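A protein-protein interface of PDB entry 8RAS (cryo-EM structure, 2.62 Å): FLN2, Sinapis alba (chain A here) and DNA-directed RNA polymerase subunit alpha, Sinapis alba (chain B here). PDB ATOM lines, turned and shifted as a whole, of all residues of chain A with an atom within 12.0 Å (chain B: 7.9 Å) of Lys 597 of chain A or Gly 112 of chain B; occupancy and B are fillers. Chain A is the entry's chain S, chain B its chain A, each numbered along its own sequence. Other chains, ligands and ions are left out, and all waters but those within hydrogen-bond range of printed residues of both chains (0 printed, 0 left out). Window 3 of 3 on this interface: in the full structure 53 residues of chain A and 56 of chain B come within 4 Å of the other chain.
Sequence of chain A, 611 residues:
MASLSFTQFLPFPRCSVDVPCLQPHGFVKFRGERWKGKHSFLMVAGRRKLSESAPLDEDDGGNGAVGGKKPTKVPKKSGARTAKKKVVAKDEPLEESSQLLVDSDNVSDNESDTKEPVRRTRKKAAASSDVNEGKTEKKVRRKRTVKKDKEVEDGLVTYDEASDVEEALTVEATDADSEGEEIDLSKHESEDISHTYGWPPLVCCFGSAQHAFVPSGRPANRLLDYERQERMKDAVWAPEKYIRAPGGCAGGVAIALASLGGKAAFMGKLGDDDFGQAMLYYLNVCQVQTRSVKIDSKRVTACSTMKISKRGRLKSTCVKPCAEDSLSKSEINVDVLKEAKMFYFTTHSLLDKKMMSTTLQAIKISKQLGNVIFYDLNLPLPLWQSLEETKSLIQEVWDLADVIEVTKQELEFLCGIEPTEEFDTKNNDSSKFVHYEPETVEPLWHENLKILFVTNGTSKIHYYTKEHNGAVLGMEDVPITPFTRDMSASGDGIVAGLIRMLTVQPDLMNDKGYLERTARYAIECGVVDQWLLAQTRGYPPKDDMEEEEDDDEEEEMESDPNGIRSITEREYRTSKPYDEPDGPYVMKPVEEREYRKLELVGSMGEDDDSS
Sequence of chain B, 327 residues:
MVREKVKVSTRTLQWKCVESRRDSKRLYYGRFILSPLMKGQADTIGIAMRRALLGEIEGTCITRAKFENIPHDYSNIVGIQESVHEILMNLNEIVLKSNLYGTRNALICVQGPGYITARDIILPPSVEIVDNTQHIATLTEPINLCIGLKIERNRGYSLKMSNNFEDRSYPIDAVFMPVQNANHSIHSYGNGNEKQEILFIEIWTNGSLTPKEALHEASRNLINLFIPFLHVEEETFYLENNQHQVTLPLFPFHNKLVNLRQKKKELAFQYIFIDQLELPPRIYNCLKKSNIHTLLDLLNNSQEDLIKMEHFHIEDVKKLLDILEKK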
ATOM      1  N   ARG A 593     -10.926   8.478 -13.115  1.00  0.00           N
ATOM      2  CA  ARG A 593     -10.748   9.266 -11.901  1.00  0.00           C
ATOM      3  C   ARG A 593     -11.936  10.163 -11.596  1.00  0.00           C
ATOM      4  O   ARG A 593     -12.441  10.146 -10.466  1.00  0.00           O
ATOM      5  CB  ARG A 593      -9.465  10.104 -12.005  1.00  0.00           C
ATOM      6  CG  ARG A 593      -8.220   9.384 -11.513  1.00  0.00           C
ATOM      7  CD  ARG A 593      -8.251   9.192 -10.004  1.00  0.00           C
ATOM      8  NE  ARG A 593      -7.156   8.349  -9.535  1.00  0.00           N
ATOM      9  CZ  ARG A 593      -5.924   8.780  -9.305  1.00  0.00           C
ATOM     10  NH1 ARG A 593      -5.589  10.047  -9.487  1.00  0.00           N
ATOM     11  NH2 ARG A 593      -5.004   7.918  -8.883  1.00  0.00           N
ATOM     12  N   GLU A 594     -12.396  10.952 -12.570  1.00  0.00           N
ATOM     13  CA  GLU A 594     -13.545  11.849 -12.420  1.00  0.00           C
ATOM     14  C   GLU A 594     -13.315  12.861 -11.292  1.00  0.00           C
ATOM     15  O   GLU A 594     -13.996  12.873 -10.264  1.00  0.00           O
ATOM     16  CB  GLU A 594     -14.839  11.056 -12.192  1.00  0.00           C
ATOM     17  CG  GLU A 594     -15.411  10.429 -13.450  1.00  0.00           C
ATOM     18  CD  GLU A 594     -14.939   9.006 -13.651  1.00  0.00           C
ATOM     19  OE1 GLU A 594     -14.217   8.494 -12.770  1.00  0.00           O
ATOM     20  OE2 GLU A 594     -15.289   8.398 -14.685  1.00  0.00           O
ATOM     21  N   TYR A 595     -12.319  13.715 -11.518  1.00  0.00           N
ATOM     22  CA  TYR A 595     -12.068  14.826 -10.611  1.00  0.00           C
ATOM     23  C   TYR A 595     -13.236  15.806 -10.634  1.00  0.00           C
ATOM     24  O   TYR A 595     -13.890  16.006 -11.662  1.00  0.00           O
ATOM     25  CB  TYR A 595     -10.781  15.554 -11.000  1.00  0.00           C
ATOM     26  CG  TYR A 595      -9.536  14.701 -10.950  1.00  0.00           C
ATOM     27  CD1 TYR A 595      -9.477  13.569 -10.154  1.00  0.00           C
ATOM     28  CD2 TYR A 595      -8.424  15.021 -11.715  1.00  0.00           C
ATOM     29  CE1 TYR A 595      -8.342  12.786 -10.109  1.00  0.00           C
ATOM     30  CE2 TYR A 595      -7.287  14.242 -11.680  1.00  0.00           C
ATOM     31  CZ  TYR A 595      -7.250  13.126 -10.874  1.00  0.00           C
ATOM     32  OH  TYR A 595      -6.119  12.344 -10.832  1.00  0.00           O
ATOM     33  N   ARG A 596     -13.498  16.421  -9.485  1.00  0.00           N
ATOM     34  CA  ARG A 596     -14.495  17.475  -9.366  1.00  0.00           C
ATOM     35  C   ARG A 596     -13.785  18.804  -9.152  1.00  0.00           C
ATOM     36  O   ARG A 596     -12.868  18.899  -8.330  1.00  0.00           O
ATOM     37  CB  ARG A 596     -15.472  17.194  -8.222  1.00  0.00           C
ATOM     38  CG  ARG A 596     -14.813  16.847  -6.900  1.00  0.00           C
ATOM     39  CD  ARG A 596     -15.843  16.464  -5.850  1.00  0.00           C
ATOM     40  NE  ARG A 596     -16.326  17.628  -5.115  1.00  0.00           N
ATOM     41  CZ  ARG A 596     -17.220  17.578  -4.137  1.00  0.00           C
ATOM     42  NH1 ARG A 596     -17.754  16.434  -3.746  1.00  0.00           N
ATOM     43  NH2 ARG A 596     -17.586  18.707  -3.536  1.00  0.00           N
ATOM     44  N   LYS A 597     -14.201  19.821  -9.903  1.00  0.00           N
ATOM     45  CA  LYS A 597     -13.546  21.118  -9.830  1.00  0.00           C
ATOM     46  C   LYS A 597     -13.888  21.825  -8.525  1.00  0.00           C
ATOM     47  O   LYS A 597     -15.020  21.754  -8.037  1.00  0.00           O
ATOM     48  CB  LYS A 597     -13.953  21.985 -11.021  1.00  0.00           C
ATOM     49  CG  LYS A 597     -12.933  23.048 -11.391  1.00  0.00           C
ATOM     50  CD  LYS A 597     -11.610  22.422 -11.805  1.00  0.00           C
ATOM     51  CE  LYS A 597     -10.669  23.460 -12.394  1.00  0.00           C
ATOM     52  NZ  LYS A 597      -9.408  22.848 -12.898  1.00  0.00           N
ATOM     53  N   LEU A 598     -12.900  22.512  -7.961  1.00  0.00           N
ATOM     54  CA  LEU A 598     -13.087  23.244  -6.715  1.00  0.00           C
ATOM     55  C   LEU A 598     -13.747  24.595  -6.965  1.00  0.00           C
ATOM     56  O   LEU A 598     -13.900  25.401  -6.046  1.00  0.00           O
ATOM     57  CB  LEU A 598     -11.747  23.435  -6.003  1.00  0.00           C
ATOM     58  CG  LEU A 598     -11.017  22.152  -5.603  1.00  0.00           C
ATOM     59  CD1 LEU A 598      -9.618  22.460  -5.100  1.00  0.00           C
ATOM     60  CD2 LEU A 598     -11.811  21.398  -4.550  1.00  0.00           C
ATOM     61  N   GLY B  79       2.596  22.938  -6.048  1.00  0.00           N
ATOM     62  CA  GLY B  79       1.260  23.432  -6.293  1.00  0.00           C
ATOM     63  C   GLY B  79       0.345  23.446  -5.087  1.00  0.00           C
ATOM     64  O   GLY B  79      -0.721  24.071  -5.150  1.00  0.00           O
ATOM     65  N   CYS B 109     -11.158  13.421  -4.127  1.00  0.00           N
ATOM     66  CA  CYS B 109     -10.777  13.349  -5.541  1.00  0.00           C
ATOM     67  C   CYS B 109     -11.194  14.663  -6.198  1.00  0.00           C
ATOM     68  O   CYS B 109     -12.311  14.789  -6.706  1.00  0.00           O
ATOM     69  CB  CYS B 109     -11.423  12.146  -6.217  1.00  0.00           C
ATOM     70  SG  CYS B 109     -10.537  11.515  -7.655  1.00  0.00           S
ATOM     71  N   VAL B 110     -10.285  15.640  -6.187  1.00  0.00           N
ATOM     72  CA  VAL B 110     -10.559  16.972  -6.708  1.00  0.00           C
ATOM     73  C   VAL B 110      -9.399  17.412  -7.590  1.00  0.00           C
ATOM     74  O   VAL B 110      -8.294  16.869  -7.525  1.00  0.00           O
ATOM     75  CB  VAL B 110     -10.784  18.009  -5.586  1.00  0.00           C
ATOM     76  CG1 VAL B 110     -12.018  17.661  -4.770  1.00  0.00           C
ATOM     77  CG2 VAL B 110      -9.559  18.097  -4.696  1.00  0.00           C
ATOM     78  N   GLN B 111      -9.668  18.414  -8.422  1.00  0.00           N
ATOM     79  CA  GLN B 111      -8.654  19.046  -9.254  1.00  0.00           C
ATOM     80  C   GLN B 111      -8.585  20.529  -8.920  1.00  0.00           C
ATOM     81  O   GLN B 111      -9.618  21.189  -8.767  1.00  0.00           O
ATOM     82  CB  GLN B 111      -8.953  18.860 -10.743  1.00  0.00           C
ATOM     83  CG  GLN B 111      -7.710  18.815 -11.612  1.00  0.00           C
ATOM     84  CD  GLN B 111      -7.892  19.537 -12.930  1.00  0.00           C
ATOM     85  OE1 GLN B 111      -8.959  20.081 -13.212  1.00  0.00           O
ATOM     86  NE2 GLN B 111      -6.844  19.551 -13.745  1.00  0.00           N
ATOM     87  N   GLY B 112      -7.365  21.049  -8.809  1.00  0.00           N
ATOM     88  CA  GLY B 112      -7.171  22.430  -8.444  1.00  0.00           C
ATOM     89  C   GLY B 112      -7.310  23.360  -9.628  1.00  0.00           C
ATOM     90  O   GLY B 112      -7.618  22.955 -10.757  1.00  0.00           O
ATOM     91  N   PRO B 113      -7.083  24.655  -9.372  1.00  0.00           N
ATOM     92  CA  PRO B 113      -6.763  25.276  -8.081  1.00  0.00           C
ATOM     93  C   PRO B 113      -8.009  25.520  -7.238  1.00  0.00           C
ATOM     94  O   PRO B 113      -9.125  25.450  -7.745  1.00  0.00           O
ATOM     95  CB  PRO B 113      -6.088  26.585  -8.502  1.00  0.00           C
ATOM     96  CG  PRO B 113      -6.809  26.959  -9.762  1.00  0.00           C
ATOM     97  CD  PRO B 113      -7.096  25.648 -10.462  1.00  0.00           C
ATOM     98  N   GLY B 114      -7.854  25.805  -5.956  1.00  0.00           N
ATOM     99  CA  GLY B 114      -8.985  26.081  -5.097  1.00  0.00           C
ATOM    100  C   GLY B 114      -8.696  25.643  -3.675  1.00  0.00           C
ATOM    101  O   GLY B 114      -7.582  25.257  -3.336  1.00  0.00           O
ATOM    102  N   TYR B 115      -9.738  25.712  -2.851  1.00  0.00           N
ATOM    103  CA  TYR B 115      -9.665  25.359  -1.440  1.00  0.00           C
ATOM    104  C   TYR B 115     -10.342  24.014  -1.217  1.00  0.00           C
ATOM    105  O   TYR B 115     -11.477  23.807  -1.657  1.00  0.00           O
ATOM    106  CB  TYR B 115     -10.329  26.430  -0.574  1.00  0.00           C
ATOM    107  CG  TYR B 115      -9.540  27.713  -0.468  1.00  0.00           C
ATOM    108  CD1 TYR B 115      -8.210  27.702  -0.077  1.00  0.00           C
ATOM    109  CD2 TYR B 115     -10.126  28.937  -0.757  1.00  0.00           C
ATOM    110  CE1 TYR B 115      -7.484  28.872   0.022  1.00  0.00           C
ATOM    111  CE2 TYR B 115      -9.409  30.114  -0.661  1.00  0.00           C
ATOM    112  CZ  TYR B 115      -8.088  30.075  -0.271  1.00  0.00           C
ATOM    113  OH  TYR B 115      -7.369  31.243  -0.175  1.00  0.00           O
ATOM    114  N   ILE B 116      -9.648  23.110  -0.537  1.00  0.00           N
ATOM    115  CA  ILE B 116     -10.175  21.790  -0.215  1.00  0.00           C
ATOM    116  C   ILE B 116     -10.739  21.849   1.197  1.00  0.00           C
ATOM    117  O   ILE B 116      -9.987  21.853   2.177  1.00  0.00           O
ATOM    118  CB  ILE B 116      -9.101  20.702  -0.339  1.00  0.00           C
ATOM    119  CG1 ILE B 116      -8.383  20.813  -1.684  1.00  0.00           C
ATOM    120  CG2 ILE B 116      -9.722  19.327  -0.171  1.00  0.00           C
ATOM    121  CD1 ILE B 116      -7.533  19.615  -2.014  1.00  0.00           C
ATOM    122  N   ASP B 120     -15.600  18.472   0.598  1.00  0.00           N
ATOM    123  CA  ASP B 120     -15.061  17.822  -0.586  1.00  0.00           C
ATOM    124  C   ASP B 120     -14.810  16.334  -0.379  1.00  0.00           C
ATOM    125  O   ASP B 120     -14.299  15.674  -1.289  1.00  0.00           O
ATOM    126  CB  ASP B 120     -13.757  18.502  -1.016  1.00  0.00           C
ATOM    127  CG  ASP B 120     -13.982  19.900  -1.551  1.00  0.00           C
ATOM    128  OD1 ASP B 120     -15.115  20.201  -1.977  1.00  0.00           O
ATOM    129  OD2 ASP B 120     -13.022  20.699  -1.546  1.00  0.00           O
ATOM    130  N   THR B 138      -4.953  23.851   0.301  1.00  0.00           N
ATOM    131  CA  THR B 138      -5.249  24.802  -0.761  1.00  0.00           C
ATOM    132  C   THR B 138      -4.410  24.466  -1.986  1.00  0.00           C
ATOM    133  O   THR B 138      -3.208  24.207  -1.873  1.00  0.00           O
ATOM    134  CB  THR B 138      -4.999  26.247  -0.308  1.00  0.00           C
ATOM    135  OG1 THR B 138      -5.257  27.144  -1.395  1.00  0.00           O
ATOM    136  CG2 THR B 138      -3.574  26.438   0.189  1.00  0.00           C
ATOM    137  N   LEU B 139      -5.055  24.444  -3.148  1.00  0.00           N
ATOM    138  CA  LEU B 139      -4.390  24.163  -4.413  1.00  0.00           C
ATOM    139  C   LEU B 139      -4.185  25.476  -5.159  1.00  0.00           C
ATOM    140  O   LEU B 139      -5.147  26.210  -5.407  1.00  0.00           O
ATOM    141  CB  LEU B 139      -5.210  23.185  -5.252  1.00  0.00           C
ATOM    142  CG  LEU B 139      -4.997  21.696  -4.968  1.00  0.00           C
ATOM    143  CD1 LEU B 139      -6.270  20.914  -5.234  1.00  0.00           C
ATOM    144  CD2 LEU B 139      -3.855  21.153  -5.807  1.00  0.00           C
ATOM    145  N   THR B 140      -2.934  25.772  -5.505  1.00  0.00           N
ATOM    146  CA  THR B 140      -2.614  27.008  -6.207  1.00  0.00           C
ATOM    147  C   THR B 140      -2.672  26.858  -7.720  1.00  0.00           C
ATOM    148  O   THR B 140      -2.962  27.834  -8.422  1.00  0.00           O
ATOM    149  CB  THR B 140      -1.224  27.503  -5.799  1.00  0.00           C
ATOM    150  OG1 THR B 140      -0.350  26.382  -5.620  1.00  0.00           O
ATOM    151  CG2 THR B 140      -1.302  28.287  -4.500  1.00  0.00           C
ATOM    152  N   GLU B 141      -2.408  25.665  -8.233  1.00  0.00           N
ATOM    153  CA  GLU B 141      -2.407  25.358  -9.655  1.00  0.00           C
ATOM    154  C   GLU B 141      -3.254  24.121  -9.888  1.00  0.00           C
ATOM    155  O   GLU B 141      -3.618  23.416  -8.941  1.00  0.00           O
ATOM    156  CB  GLU B 141      -0.972  25.136 -10.164  1.00  0.00           C
ATOM    157  CG  GLU B 141       0.109  25.780  -9.314  1.00  0.00           C
ATOM    158  CD  GLU B 141       1.502  25.502  -9.840  1.00  0.00           C
ATOM    159  OE1 GLU B 141       1.811  24.323 -10.112  1.00  0.00           O
ATOM    160  OE2 GLU B 141       2.289  26.461  -9.980  1.00  0.00           O
ATOM    161  N   PRO B 142      -3.626  23.838 -11.143  1.00  0.00           N
ATOM    162  CA  PRO B 142      -4.393  22.597 -11.405  1.00  0.00           C
ATOM    163  C   PRO B 142      -3.545  21.326 -11.415  1.00  0.00           C
ATOM    164  O   PRO B 142      -3.109  20.820 -12.449  1.00  0.00           O
ATOM    165  CB  PRO B 142      -5.023  22.869 -12.776  1.00  0.00           C
ATOM    166  CG  PRO B 142      -4.731  24.306 -13.108  1.00  0.00           C
ATOM    167  CD  PRO B 142      -3.519  24.678 -12.346  1.00  0.00           C
ATOM    168  N   ILE B 143      -3.297  20.785 -10.223  1.00  0.00           N
ATOM    169  CA  ILE B 143      -2.652  19.486 -10.074  1.00  0.00           C
ATOM    170  C   ILE B 143      -3.696  18.496  -9.577  1.00  0.00           C
ATOM    171  O   ILE B 143      -4.616  18.849  -8.831  1.00  0.00           O
ATOM    172  CB  ILE B 143      -1.425  19.474  -9.127  1.00  0.00           C
ATOM    173  CG1 ILE B 143      -0.486  20.665  -9.349  1.00  0.00           C
ATOM    174  CG2 ILE B 143      -0.631  18.183  -9.276  1.00  0.00           C
ATOM    175  CD1 ILE B 143      -0.916  21.942  -8.695  1.00  0.00           C
ATOM    176  N   ASN B 144      -3.554  17.248 -10.013  1.00  0.00           N
ATOM    177  CA  ASN B 144      -4.402  16.174  -9.516  1.00  0.00           C
ATOM    178  C   ASN B 144      -4.089  15.882  -8.054  1.00  0.00           C
ATOM    179  O   ASN B 144      -2.931  15.926  -7.629  1.00  0.00           O
ATOM    180  CB  ASN B 144      -4.197  14.914 -10.354  1.00  0.00           C
ATOM    181  CG  ASN B 144      -3.964  15.222 -11.818  1.00  0.00           C
ATOM    182  OD1 ASN B 144      -4.650  16.059 -12.405  1.00  0.00           O
ATOM    183  ND2 ASN B 144      -2.990  14.548 -12.419  1.00  0.00           N
ATOM    184  N   LEU B 145      -5.131  15.585  -7.280  1.00  0.00           N
ATOM    185  CA  LEU B 145      -4.971  15.208  -5.879  1.00  0.00           C
ATOM    186  C   LEU B 145      -6.026  14.174  -5.526  1.00  0.00           C
ATOM    187  O   LEU B 145      -7.223  14.476  -5.540  1.00  0.00           O
ATOM    188  CB  LEU B 145      -5.080  16.424  -4.956  1.00  0.00           C
ATOM    189  CG  LEU B 145      -4.526  16.213  -3.545  1.00  0.00           C
ATOM    190  CD1 LEU B 145      -3.074  15.759  -3.600  1.00  0.00           C
ATOM    191  CD2 LEU B 145      -4.659  17.478  -2.717  1.00  0.00           C
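SG of Cys 109 of chain B sits at hydrogen-bond distance from O of Arg 593 of chain A, 3.7 Å away. The backbone NH (N) of Arg 596 of chain A lies close to the backbone carbonyl oxygen (O) of Cys 109 of chain B, at 3.4 Å. N of Gln 111 of chain B is in hydrogen-bond range of O of Arg 596 of chain A, 3.2 Å away. The side-chain amide oxygen (OE1) of Gln 111 of chain B sits at hydrogen-bond distance from the side-chain amino group (NZ) of Lys 597 of chain A, at 2.8 Å. NZ of Lys 597 of chain A sits at hydrogen-bond distance from O of Gly 112 of chain B (2.8 Å). The side-chain carboxylate of Asp 120 of chain B lies within salt-bridge range of the guanidinium group of Arg 596 of chain A (3.3 Å).
The backbone carbonyl oxygen of Leu 145 of chain B is in hydrogen-bond range of the backbone NH of Val 110 of chain B (3.3 Å). The backbone NH of Leu 139 of chain B lies within hydrogen-bond range of the backbone carbonyl oxygen of Gly 114 of chain B (2.7 Å). The guanidinium group (NH1) of Arg 593 of chain A sits at hydrogen-bond distance from the side-chain hydroxyl (OH) of Tyr 595 of chain A, 2.7 Å away.
Cys 109 of chain B touches Tyr 595 of chain A (SG to CD1, 3.4 Å). CB of Gln 111 of chain B touches CB of Tyr 595 of chain A, 3.8 Å away. Val 110 of chain B touches Leu 598 of chain A (CB to CD2, 3.7 Å). Leu 598 of chain A touches Gln 111 of chain B (CG to O, 3.6 Å). Leu 598 of chain A touches Pro 113 of chain B (CB to O, 3.7 Å). Gly 114 of chain B touches Leu 598 of chain A. CD2 of Leu 598 of chain A touches O of Tyr 115 of chain B, at 3.8 Å. Leu 598 of chain A touches Ile 116 of chain B (CD1 to CG1, 3.99 Å). Leu 598 of chain A touches Asp 120 of chain B (CD2 to OD2, 3.3 Å). Leu 139 of chain B touches Leu 598 of chain A.
Printed residues of chain B within 4 Å of Tyr 595 of chain A: Cys 109, Gln 111 and Asn 144. Of chain B, only Gln 111 (2.8 Å) and Gly 112 (2.8 Å) come within 4 Å of Lys 597 of chain A. Val 110 of chain B touches two residues of chain A. Gln 111 of chain B touches four residues of chain A. Gly 112 of chain B touches one residue of chain A. Of chain A, only Leu 598 comes within 4 Å of Gly 114 of chain B. Of the printed residues of chain A, Ile 116 of chain B touches Leu 598. Of the printed residues of chain A, Asp 120 of chain B touches Arg 596 (3.3 Å) and Leu 598 (3.3 Å). Thr 138 of chain B touches none of the printed residues of chain A. No residue of chain A comes within 4 Å of Ile 143 of chain B. Of the printed residues of chain A, Asn 144 of chain B touches Tyr 595. The nearest printed residue of chain B that does not touch Lys 597 of chain A is Pro 113 of chain B (4.4 Å).
Printed residues of chain A that touch a printed residue of chain B: Arg 593, Tyr 595, Arg 596, Lys 597 and Leu 598. Hydrophobic or aromatic side chains of chain A that line the printed part of chain B: Tyr 595 and Leu 598. Along chain A the printed residues that touch a printed residue of chain B span positions 593 to 598. Of the 18 printed residues of chain B, 11 touch a printed residue of chain A. Hydrophobic or aromatic side chains of chain B within 4 Å of the printed part of chain A: Val 110, Ile 116 and Leu 139. Along chain B the printed residues that touch a printed residue of chain A span positions 109 to 144. Among the printed residues, 18 pairs touch across the chains. Among the printed residues, Asp or Glu carboxylates within 4 Å of a Lys or Arg side-chain nitrogen of the other chain: Arg 596 of chain A with Asp 120 of chain B.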
